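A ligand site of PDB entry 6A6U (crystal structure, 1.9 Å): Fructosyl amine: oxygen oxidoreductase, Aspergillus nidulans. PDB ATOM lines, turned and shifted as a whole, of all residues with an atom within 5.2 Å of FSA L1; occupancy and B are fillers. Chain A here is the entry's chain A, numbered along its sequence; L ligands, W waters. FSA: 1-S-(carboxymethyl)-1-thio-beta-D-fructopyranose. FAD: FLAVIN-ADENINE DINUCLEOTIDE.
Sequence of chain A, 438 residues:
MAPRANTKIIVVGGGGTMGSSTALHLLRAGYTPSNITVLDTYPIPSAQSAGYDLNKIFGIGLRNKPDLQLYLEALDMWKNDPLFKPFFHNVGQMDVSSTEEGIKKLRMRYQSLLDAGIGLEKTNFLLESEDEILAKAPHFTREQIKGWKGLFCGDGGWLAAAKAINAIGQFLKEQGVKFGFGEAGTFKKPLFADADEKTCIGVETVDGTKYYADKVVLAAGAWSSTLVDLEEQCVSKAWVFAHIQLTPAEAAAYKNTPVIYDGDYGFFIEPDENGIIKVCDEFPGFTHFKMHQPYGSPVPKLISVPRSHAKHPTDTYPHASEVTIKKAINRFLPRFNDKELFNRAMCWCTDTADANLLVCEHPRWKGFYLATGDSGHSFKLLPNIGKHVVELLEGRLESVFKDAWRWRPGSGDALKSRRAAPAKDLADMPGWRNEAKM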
ATOM      1  N   ILE A  57     -25.361  28.774  11.257  1.00  0.00           N
ATOM      2  CA  ILE A  57     -24.157  29.419  11.765  1.00  0.00           C
ATOM      3  C   ILE A  57     -22.960  29.202  10.843  1.00  0.00           C
ATOM      4  O   ILE A  57     -22.782  28.102  10.303  1.00  0.00           O
ATOM      5  CB  ILE A  57     -23.779  28.890  13.153  1.00  0.00           C
ATOM      6  CG1 ILE A  57     -24.968  28.997  14.098  1.00  0.00           C
ATOM      7  CG2 ILE A  57     -22.577  29.631  13.715  1.00  0.00           C
ATOM      8  CD1 ILE A  57     -24.706  28.319  15.427  1.00  0.00           C
ATOM      9  N   PHE A  58     -22.152  30.250  10.672  1.00  0.00           N
ATOM     10  CA  PHE A  58     -20.836  30.077  10.062  1.00  0.00           C
ATOM     11  C   PHE A  58     -19.782  30.270  11.137  1.00  0.00           C
ATOM     12  O   PHE A  58     -19.645  31.352  11.694  1.00  0.00           O
ATOM     13  CB  PHE A  58     -20.566  31.074   8.930  1.00  0.00           C
ATOM     14  CG  PHE A  58     -19.230  30.849   8.252  1.00  0.00           C
ATOM     15  CD1 PHE A  58     -19.087  29.882   7.284  1.00  0.00           C
ATOM     16  CD2 PHE A  58     -18.110  31.570   8.632  1.00  0.00           C
ATOM     17  CE1 PHE A  58     -17.865  29.639   6.684  1.00  0.00           C
ATOM     18  CE2 PHE A  58     -16.880  31.345   8.027  1.00  0.00           C
ATOM     19  CZ  PHE A  58     -16.759  30.376   7.059  1.00  0.00           C
ATOM     20  N   GLY A  59     -19.036  29.226  11.429  1.00  0.00           N
ATOM     21  CA  GLY A  59     -18.064  29.313  12.484  1.00  0.00           C
ATOM     22  C   GLY A  59     -16.902  28.385  12.220  1.00  0.00           C
ATOM     23  O   GLY A  59     -16.991  27.498  11.372  1.00  0.00           O
ATOM     24  N   TRP A 239     -32.015  16.816  13.976  1.00  0.00           N
ATOM     25  CA  TRP A 239     -31.917  17.861  14.984  1.00  0.00           C
ATOM     26  C   TRP A 239     -33.170  18.710  14.864  1.00  0.00           C
ATOM     27  O   TRP A 239     -33.982  18.503  13.972  1.00  0.00           O
ATOM     28  CB  TRP A 239     -30.626  18.679  14.812  1.00  0.00           C
ATOM     29  CG  TRP A 239     -29.501  17.929  15.413  1.00  0.00           C
ATOM     30  CD1 TRP A 239     -29.030  18.051  16.696  1.00  0.00           C
ATOM     31  CD2 TRP A 239     -28.752  16.861  14.813  1.00  0.00           C
ATOM     32  NE1 TRP A 239     -28.010  17.158  16.901  1.00  0.00           N
ATOM     33  CE2 TRP A 239     -27.823  16.417  15.770  1.00  0.00           C
ATOM     34  CE3 TRP A 239     -28.753  16.260  13.544  1.00  0.00           C
ATOM     35  CZ2 TRP A 239     -26.914  15.393  15.502  1.00  0.00           C
ATOM     36  CZ3 TRP A 239     -27.841  15.248  13.283  1.00  0.00           C
ATOM     37  CH2 TRP A 239     -26.936  14.832  14.262  1.00  0.00           C
ATOM     38  N   TYR A 261     -23.942  30.632  21.676  1.00  0.00           N
ATOM     39  CA  TYR A 261     -23.945  29.163  21.782  1.00  0.00           C
ATOM     40  C   TYR A 261     -23.442  28.696  23.141  1.00  0.00           C
ATOM     41  O   TYR A 261     -22.471  29.217  23.655  1.00  0.00           O
ATOM     42  CB  TYR A 261     -23.063  28.553  20.686  1.00  0.00           C
ATOM     43  CG  TYR A 261     -22.988  27.035  20.703  1.00  0.00           C
ATOM     44  CD1 TYR A 261     -22.046  26.371  21.476  1.00  0.00           C
ATOM     45  CD2 TYR A 261     -23.847  26.271  19.919  1.00  0.00           C
ATOM     46  CE1 TYR A 261     -21.975  24.977  21.486  1.00  0.00           C
ATOM     47  CE2 TYR A 261     -23.785  24.878  19.918  1.00  0.00           C
ATOM     48  CZ  TYR A 261     -22.846  24.241  20.703  1.00  0.00           C
ATOM     49  OH  TYR A 261     -22.799  22.866  20.707  1.00  0.00           O
ATOM     50  N   PHE A 267     -28.406  27.096  20.932  1.00  0.00           N
ATOM     51  CA  PHE A 267     -28.054  28.423  20.442  1.00  0.00           C
ATOM     52  C   PHE A 267     -29.227  29.175  19.892  1.00  0.00           C
ATOM     53  O   PHE A 267     -30.291  28.588  19.660  1.00  0.00           O
ATOM     54  CB  PHE A 267     -26.949  28.313  19.372  1.00  0.00           C
ATOM     55  CG  PHE A 267     -27.331  27.478  18.173  1.00  0.00           C
ATOM     56  CD1 PHE A 267     -28.022  28.026  17.112  1.00  0.00           C
ATOM     57  CD2 PHE A 267     -26.960  26.135  18.105  1.00  0.00           C
ATOM     58  CE1 PHE A 267     -28.367  27.255  15.987  1.00  0.00           C
ATOM     59  CE2 PHE A 267     -27.299  25.351  16.984  1.00  0.00           C
ATOM     60  CZ  PHE A 267     -27.996  25.918  15.939  1.00  0.00           C
ATOM     61  N   CYS A 280     -32.218  26.513  18.562  1.00  0.00           N
ATOM     62  CA  CYS A 280     -31.933  25.081  18.563  1.00  0.00           C
ATOM     63  C   CYS A 280     -31.427  24.683  19.932  1.00  0.00           C
ATOM     64  O   CYS A 280     -30.796  25.490  20.608  1.00  0.00           O
ATOM     65  CB  CYS A 280     -30.865  24.698  17.545  1.00  0.00           C
ATOM     66  SG  CYS A 280     -31.287  24.955  15.833  1.00  0.00           S
ATOM     67  N   ASP A 281     -31.669  23.441  20.333  1.00  0.00           N
ATOM     68  CA  ASP A 281     -31.030  22.910  21.524  1.00  0.00           C
ATOM     69  C   ASP A 281     -29.704  22.269  21.099  1.00  0.00           C
ATOM     70  O   ASP A 281     -29.296  22.426  19.965  1.00  0.00           O
ATOM     71  CB  ASP A 281     -31.959  21.924  22.251  1.00  0.00           C
ATOM     72  CG  ASP A 281     -32.343  20.721  21.395  1.00  0.00           C
ATOM     73  OD1 ASP A 281     -32.007  20.675  20.197  1.00  0.00           O
ATOM     74  OD2 ASP A 281     -32.979  19.795  21.948  1.00  0.00           O
ATOM     75  N   GLU A 282     -29.023  21.590  22.012  1.00  0.00           N
ATOM     76  CA  GLU A 282     -27.867  20.769  21.610  1.00  0.00           C
ATOM     77  C   GLU A 282     -28.028  19.378  22.193  1.00  0.00           C
ATOM     78  O   GLU A 282     -28.265  19.236  23.396  1.00  0.00           O
ATOM     79  CB  GLU A 282     -26.540  21.380  22.066  1.00  0.00           C
ATOM     80  CG  GLU A 282     -25.311  20.591  21.613  1.00  0.00           C
ATOM     81  CD  GLU A 282     -25.222  20.473  20.091  1.00  0.00           C
ATOM     82  OE1 GLU A 282     -25.854  19.533  19.530  1.00  0.00           O
ATOM     83  OE2 GLU A 282     -24.555  21.314  19.449  1.00  0.00           O
ATOM     84  N   PHE A 283     -27.914  18.351  21.358  1.00  0.00           N
ATOM     85  CA  PHE A 283     -28.124  16.983  21.798  1.00  0.00           C
ATOM     86  C   PHE A 283     -27.592  16.057  20.693  1.00  0.00           C
ATOM     87  O   PHE A 283     -27.212  16.553  19.632  1.00  0.00           O
ATOM     88  CB  PHE A 283     -29.623  16.759  22.111  1.00  0.00           C
ATOM     89  CG  PHE A 283     -30.489  16.531  20.890  1.00  0.00           C
ATOM     90  CD1 PHE A 283     -30.705  17.542  19.972  1.00  0.00           C
ATOM     91  CD2 PHE A 283     -31.112  15.312  20.686  1.00  0.00           C
ATOM     92  CE1 PHE A 283     -31.522  17.334  18.850  1.00  0.00           C
ATOM     93  CE2 PHE A 283     -31.923  15.099  19.587  1.00  0.00           C
ATOM     94  CZ  PHE A 283     -32.126  16.111  18.658  1.00  0.00           C
ATOM     95  N   CYS A 349     -29.589  15.234   9.043  1.00  0.00           N
ATOM     96  CA  CYS A 349     -28.199  15.136   8.598  1.00  0.00           C
ATOM     97  C   CYS A 349     -27.769  13.677   8.640  1.00  0.00           C
ATOM     98  O   CYS A 349     -28.518  12.828   9.138  1.00  0.00           O
ATOM     99  CB  CYS A 349     -27.271  15.973   9.496  1.00  0.00           C
ATOM    100  SG  CYS A 349     -27.800  17.672   9.694  1.00  0.00           S
ATOM    101  N   SER A 375     -22.425  15.217   8.296  1.00  0.00           N
ATOM    102  CA  SER A 375     -22.201  15.144   9.742  1.00  0.00           C
ATOM    103  C   SER A 375     -22.668  16.383  10.521  1.00  0.00           C
ATOM    104  O   SER A 375     -22.106  16.689  11.570  1.00  0.00           O
ATOM    105  CB  SER A 375     -20.719  14.877  10.019  1.00  0.00           C
ATOM    106  OG  SER A 375     -20.365  13.594   9.494  1.00  0.00           O
ATOM    107  N   GLY A 376     -23.680  17.089  10.007  1.00  0.00           N
ATOM    108  CA  GLY A 376     -24.328  18.152  10.734  1.00  0.00           C
ATOM    109  C   GLY A 376     -23.550  19.441  10.865  1.00  0.00           C
ATOM    110  O   GLY A 376     -23.889  20.297  11.678  1.00  0.00           O
ATOM    111  N   HIS A 377     -22.500  19.604  10.056  1.00  0.00           N
ATOM    112  CA  HIS A 377     -21.670  20.793  10.156  1.00  0.00           C
ATOM    113  C   HIS A 377     -21.259  21.330   8.790  1.00  0.00           C
ATOM    114  O   HIS A 377     -20.262  22.027   8.695  1.00  0.00           O
ATOM    115  CB  HIS A 377     -20.405  20.506  10.992  1.00  0.00           C
ATOM    116  CG  HIS A 377     -20.661  19.984  12.365  1.00  0.00           C
ATOM    117  ND1 HIS A 377     -21.184  20.765  13.378  1.00  0.00           N
ATOM    118  CD2 HIS A 377     -20.449  18.760  12.908  1.00  0.00           C
ATOM    119  CE1 HIS A 377     -21.291  20.039  14.479  1.00  0.00           C
ATOM    120  NE2 HIS A 377     -20.851  18.815  14.229  1.00  0.00           N
ATOM    121  N   LYS A 380     -22.064  25.475   6.102  1.00  0.00           N
ATOM    122  CA  LYS A 380     -21.086  26.533   5.907  1.00  0.00           C
ATOM    123  C   LYS A 380     -20.189  26.283   4.680  1.00  0.00           C
ATOM    124  O   LYS A 380     -19.552  27.206   4.191  1.00  0.00           O
ATOM    125  CB  LYS A 380     -20.213  26.678   7.164  1.00  0.00           C
ATOM    126  CG  LYS A 380     -19.425  25.430   7.509  1.00  0.00           C
ATOM    127  CD  LYS A 380     -18.377  25.717   8.586  1.00  0.00           C
ATOM    128  CE  LYS A 380     -18.281  24.590   9.581  1.00  0.00           C
ATOM    129  NZ  LYS A 380     -19.501  24.615  10.436  1.00  0.00           N
ATOM    130  N   ARG A 419     -20.204  12.589  18.872  1.00  0.00           N
ATOM    131  CA  ARG A 419     -21.158  13.226  19.771  1.00  0.00           C
ATOM    132  C   ARG A 419     -21.143  12.568  21.155  1.00  0.00           C
ATOM    133  O   ARG A 419     -20.397  11.619  21.386  1.00  0.00           O
ATOM    134  CB  ARG A 419     -22.545  13.210  19.142  1.00  0.00           C
ATOM    135  CG  ARG A 419     -22.514  13.714  17.690  1.00  0.00           C
ATOM    136  CD  ARG A 419     -23.868  14.060  17.149  1.00  0.00           C
ATOM    137  NE  ARG A 419     -23.800  14.507  15.746  1.00  0.00           N
ATOM    138  CZ  ARG A 419     -23.784  15.782  15.355  1.00  0.00           C
ATOM    139  NH1 ARG A 419     -23.863  16.778  16.252  1.00  0.00           N
ATOM    140  NH2 ARG A 419     -23.729  16.063  14.056  1.00  0.00           N
HETATM  141  OAB FSA L   1     -21.039  23.558  12.626  1.00  0.00           O
HETATM  142  CAL FSA L   1     -21.364  24.679  13.107  1.00  0.00           C
HETATM  143  OAA FSA L   1     -20.635  25.700  13.142  1.00  0.00           O
HETATM  144  CAH FSA L   1     -22.769  24.788  13.715  1.00  0.00           C
HETATM  145  SAK FSA L   1     -23.660  23.196  13.541  1.00  0.00           S
HETATM  146  C1  FSA L   1     -25.264  23.557  14.364  1.00  0.00           C
HETATM  147  C2  FSA L   1     -25.991  22.237  14.682  1.00  0.00           C
HETATM  148  O2  FSA L   1     -27.322  22.509  15.116  1.00  0.00           O
HETATM  149  C3  FSA L   1     -25.229  21.457  15.752  1.00  0.00           C
HETATM  150  O3  FSA L   1     -25.150  22.269  16.967  1.00  0.00           O
HETATM  151  C4  FSA L   1     -25.894  20.151  16.055  1.00  0.00           C
HETATM  152  O4  FSA L   1     -25.060  19.462  17.003  1.00  0.00           O
HETATM  153  C5  FSA L   1     -25.949  19.351  14.763  1.00  0.00           C
HETATM  154  O5  FSA L   1     -24.601  19.136  14.280  1.00  0.00           O
HETATM  155  C6  FSA L   1     -26.734  20.135  13.713  1.00  0.00           C
HETATM  156  O6  FSA L   1     -26.065  21.419  13.490  1.00  0.00           O
HETATM  157  PA  FAD L   2     -29.191  18.288   1.947  1.00  0.00           P
HETATM  158  O1A FAD L   2     -28.885  19.665   1.891  1.00  0.00           O
HETATM  159  O2A FAD L   2     -30.199  17.932   2.773  1.00  0.00           O
HETATM  160  O5B FAD L   2     -29.423  17.739   0.524  1.00  0.00           O
HETATM  161  C5B FAD L   2     -29.882  16.477   0.261  1.00  0.00           C
HETATM  162  C4B FAD L   2     -30.930  16.483  -0.855  1.00  0.00           C
HETATM  163  O4B FAD L   2     -31.245  15.181  -1.272  1.00  0.00           O
HETATM  164  C3B FAD L   2     -32.255  17.140  -0.560  1.00  0.00           C
HETATM  165  O3B FAD L   2     -32.414  18.162  -1.471  1.00  0.00           O
HETATM  166  C2B FAD L   2     -33.293  16.056  -0.829  1.00  0.00           C
HETATM  167  O2B FAD L   2     -34.496  16.496  -1.335  1.00  0.00           O
HETATM  168  C1B FAD L   2     -32.525  15.190  -1.815  1.00  0.00           C
HETATM  169  N9A FAD L   2     -32.979  13.815  -1.960  1.00  0.00           N
HETATM  170  C8A FAD L   2     -33.315  13.002  -1.021  1.00  0.00           C
HETATM  171  N7A FAD L   2     -33.640  11.813  -1.526  1.00  0.00           N
HETATM  172  C5A FAD L   2     -33.498  11.876  -2.821  1.00  0.00           C
HETATM  173  C6A FAD L   2     -33.680  10.968  -3.945  1.00  0.00           C
HETATM  174  N6A FAD L   2     -34.076   9.758  -3.690  1.00  0.00           N
HETATM  175  N1A FAD L   2     -33.400  11.433  -5.174  1.00  0.00           N
HETATM  176  C2A FAD L   2     -32.979  12.681  -5.346  1.00  0.00           C
HETATM  177  N3A FAD L   2     -32.818  13.541  -4.375  1.00  0.00           N
HETATM  178  C4A FAD L   2     -33.035  13.198  -3.099  1.00  0.00           C
HETATM  179  N1  FAD L   2     -24.498  23.405   9.456  1.00  0.00           N
HETATM  180  C2  FAD L   2     -23.655  24.426   9.617  1.00  0.00           C
HETATM  181  O2  FAD L   2     -22.664  24.446   8.925  1.00  0.00           O
HETATM  182  N3  FAD L   2     -23.924  25.383  10.526  1.00  0.00           N
HETATM  183  C4  FAD L   2     -25.030  25.366  11.289  1.00  0.00           C
HETATM  184  O4  FAD L   2     -25.312  26.228  12.090  1.00  0.00           O
HETATM  185  C4X FAD L   2     -26.019  24.254  11.145  1.00  0.00           C
HETATM  186  N5  FAD L   2     -27.186  24.127  11.796  1.00  0.00           N
HETATM  187  C5X FAD L   2     -28.049  23.125  11.597  1.00  0.00           C
HETATM  188  C6  FAD L   2     -29.228  22.981  12.285  1.00  0.00           C
HETATM  189  C7  FAD L   2     -30.076  21.940  12.014  1.00  0.00           C
HETATM  190  C7M FAD L   2     -31.345  21.806  12.761  1.00  0.00           C
HETATM  191  C8  FAD L   2     -29.692  20.922  11.031  1.00  0.00           C
HETATM  192  C8M FAD L   2     -30.542  19.776  10.710  1.00  0.00           C
HETATM  193  C9  FAD L   2     -28.530  21.052  10.348  1.00  0.00           C
HETATM  194  C9A FAD L   2     -27.691  22.091  10.598  1.00  0.00           C
HETATM  195  N10 FAD L   2     -26.492  22.201   9.900  1.00  0.00           N
HETATM  196  C10 FAD L   2     -25.632  23.257  10.124  1.00  0.00           C
HETATM  197  C1' FAD L   2     -26.050  21.201   8.943  1.00  0.00           C
HETATM  198  C2' FAD L   2     -26.325  21.422   7.504  1.00  0.00           C
HETATM  199  O2' FAD L   2     -27.672  21.737   7.422  1.00  0.00           O
HETATM  200  C3' FAD L   2     -26.014  20.111   6.715  1.00  0.00           C
HETATM  201  O3' FAD L   2     -24.802  19.576   7.105  1.00  0.00           O
HETATM  202  C4' FAD L   2     -26.012  20.331   5.215  1.00  0.00           C
HETATM  203  O4' FAD L   2     -27.013  21.182   4.897  1.00  0.00           O
HETATM  204  C5' FAD L   2     -26.039  18.974   4.470  1.00  0.00           C
HETATM  205  O5' FAD L   2     -26.247  19.027   3.093  1.00  0.00           O
HETATM  206  P   FAD L   2     -26.540  17.806   2.232  1.00  0.00           P
HETATM  207  O1P FAD L   2     -26.430  18.315   0.946  1.00  0.00           O
HETATM  208  O2P FAD L   2     -25.684  16.751   2.643  1.00  0.00           O
HETATM  209  O3P FAD L   2     -28.054  17.501   2.591  1.00  0.00           O
HETATM  210  O   HOH W   1     -24.305  16.949  19.304  1.00  0.00           O
HETATM  211  O   HOH W   2     -28.666  21.623  17.327  1.00  0.00           O
HETATM  212  O   HOH W   3     -22.413  19.955  17.334  1.00  0.00           O
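NZ of Lys 380 is in salt-bridge range of OAB of FSA L1, 2.9 Å away.
The guanidinium group (NH1) of Arg 419 lies within hydrogen-bond range of an oxygen (O4) of FSA L1 (3.0 Å).
The backbone carbonyl oxygen of Ile 57 lies within hydrogen-bond range of a nitrogen (N3) of FAD L2 (3.0 Å).
The backbone NH of Ile 57 sits at hydrogen-bond distance from an oxygen (O4) of FAD L2 (2.7 Å).
O4 of FSA L1 lies within hydrogen-bond range of OE1 of Glu 282, 2.6 Å away.
N of Lys 380 lies within hydrogen-bond range of O2 of FAD L2 (3.1 Å).
A ring nitrogen (ND1) of His 377 lies within hydrogen-bond range of an oxygen (OAB) of FSA L1, at 2.9 Å.
An oxygen (O5) of FSA L1 lies within hydrogen-bond range of the backbone carbonyl oxygen of Gly 376 (2.9 Å).
The guanidinium group of Arg 419 is in hydrogen-bond range of the backbone carbonyl oxygen of Ser 375.
O of His 377 sits at hydrogen-bond distance from NZ of Lys 380.
NE1 of Trp 239 lies within hydrogen-bond range of O of Phe 283, at 2.9 Å.
The side-chain carboxylate (OE2) of Glu 282 lies within hydrogen-bond range of the side-chain hydroxyl (OH) of Tyr 261 (2.7 Å).
The backbone carbonyl oxygen of Cys 280 is in hydrogen-bond range of the backbone NH of Phe 267, at 2.9 Å.
A sulfur (SAK) of FSA L1 lies close to a nitrogen (N3) of FAD L2 (3.7 Å).
Water W3 bridges an oxygen (O4) of FSA L1 and the side-chain carboxylate (OE2) of Glu 282.
Water W2 lies within hydrogen-bond range of O2 of FSA L1 (2.7 Å) and O of Asp 281 (2.8 Å).
Water W1 lies within hydrogen-bond range of O of Phe 283 (3.0 Å), OE1 of Glu 282 (3.0 Å), NH1 of Arg 419 (3.1 Å) and O4 of FSA L1 (3.5 Å).
CE2 of Trp 239 touches C5 of FSA L1, 3.6 Å away.
CE2 of Phe 267 touches O2 of FSA L1 (3.4 Å).
The nearest printed residue that does not touch FSA L1 is Tyr 261 (4.2 Å).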
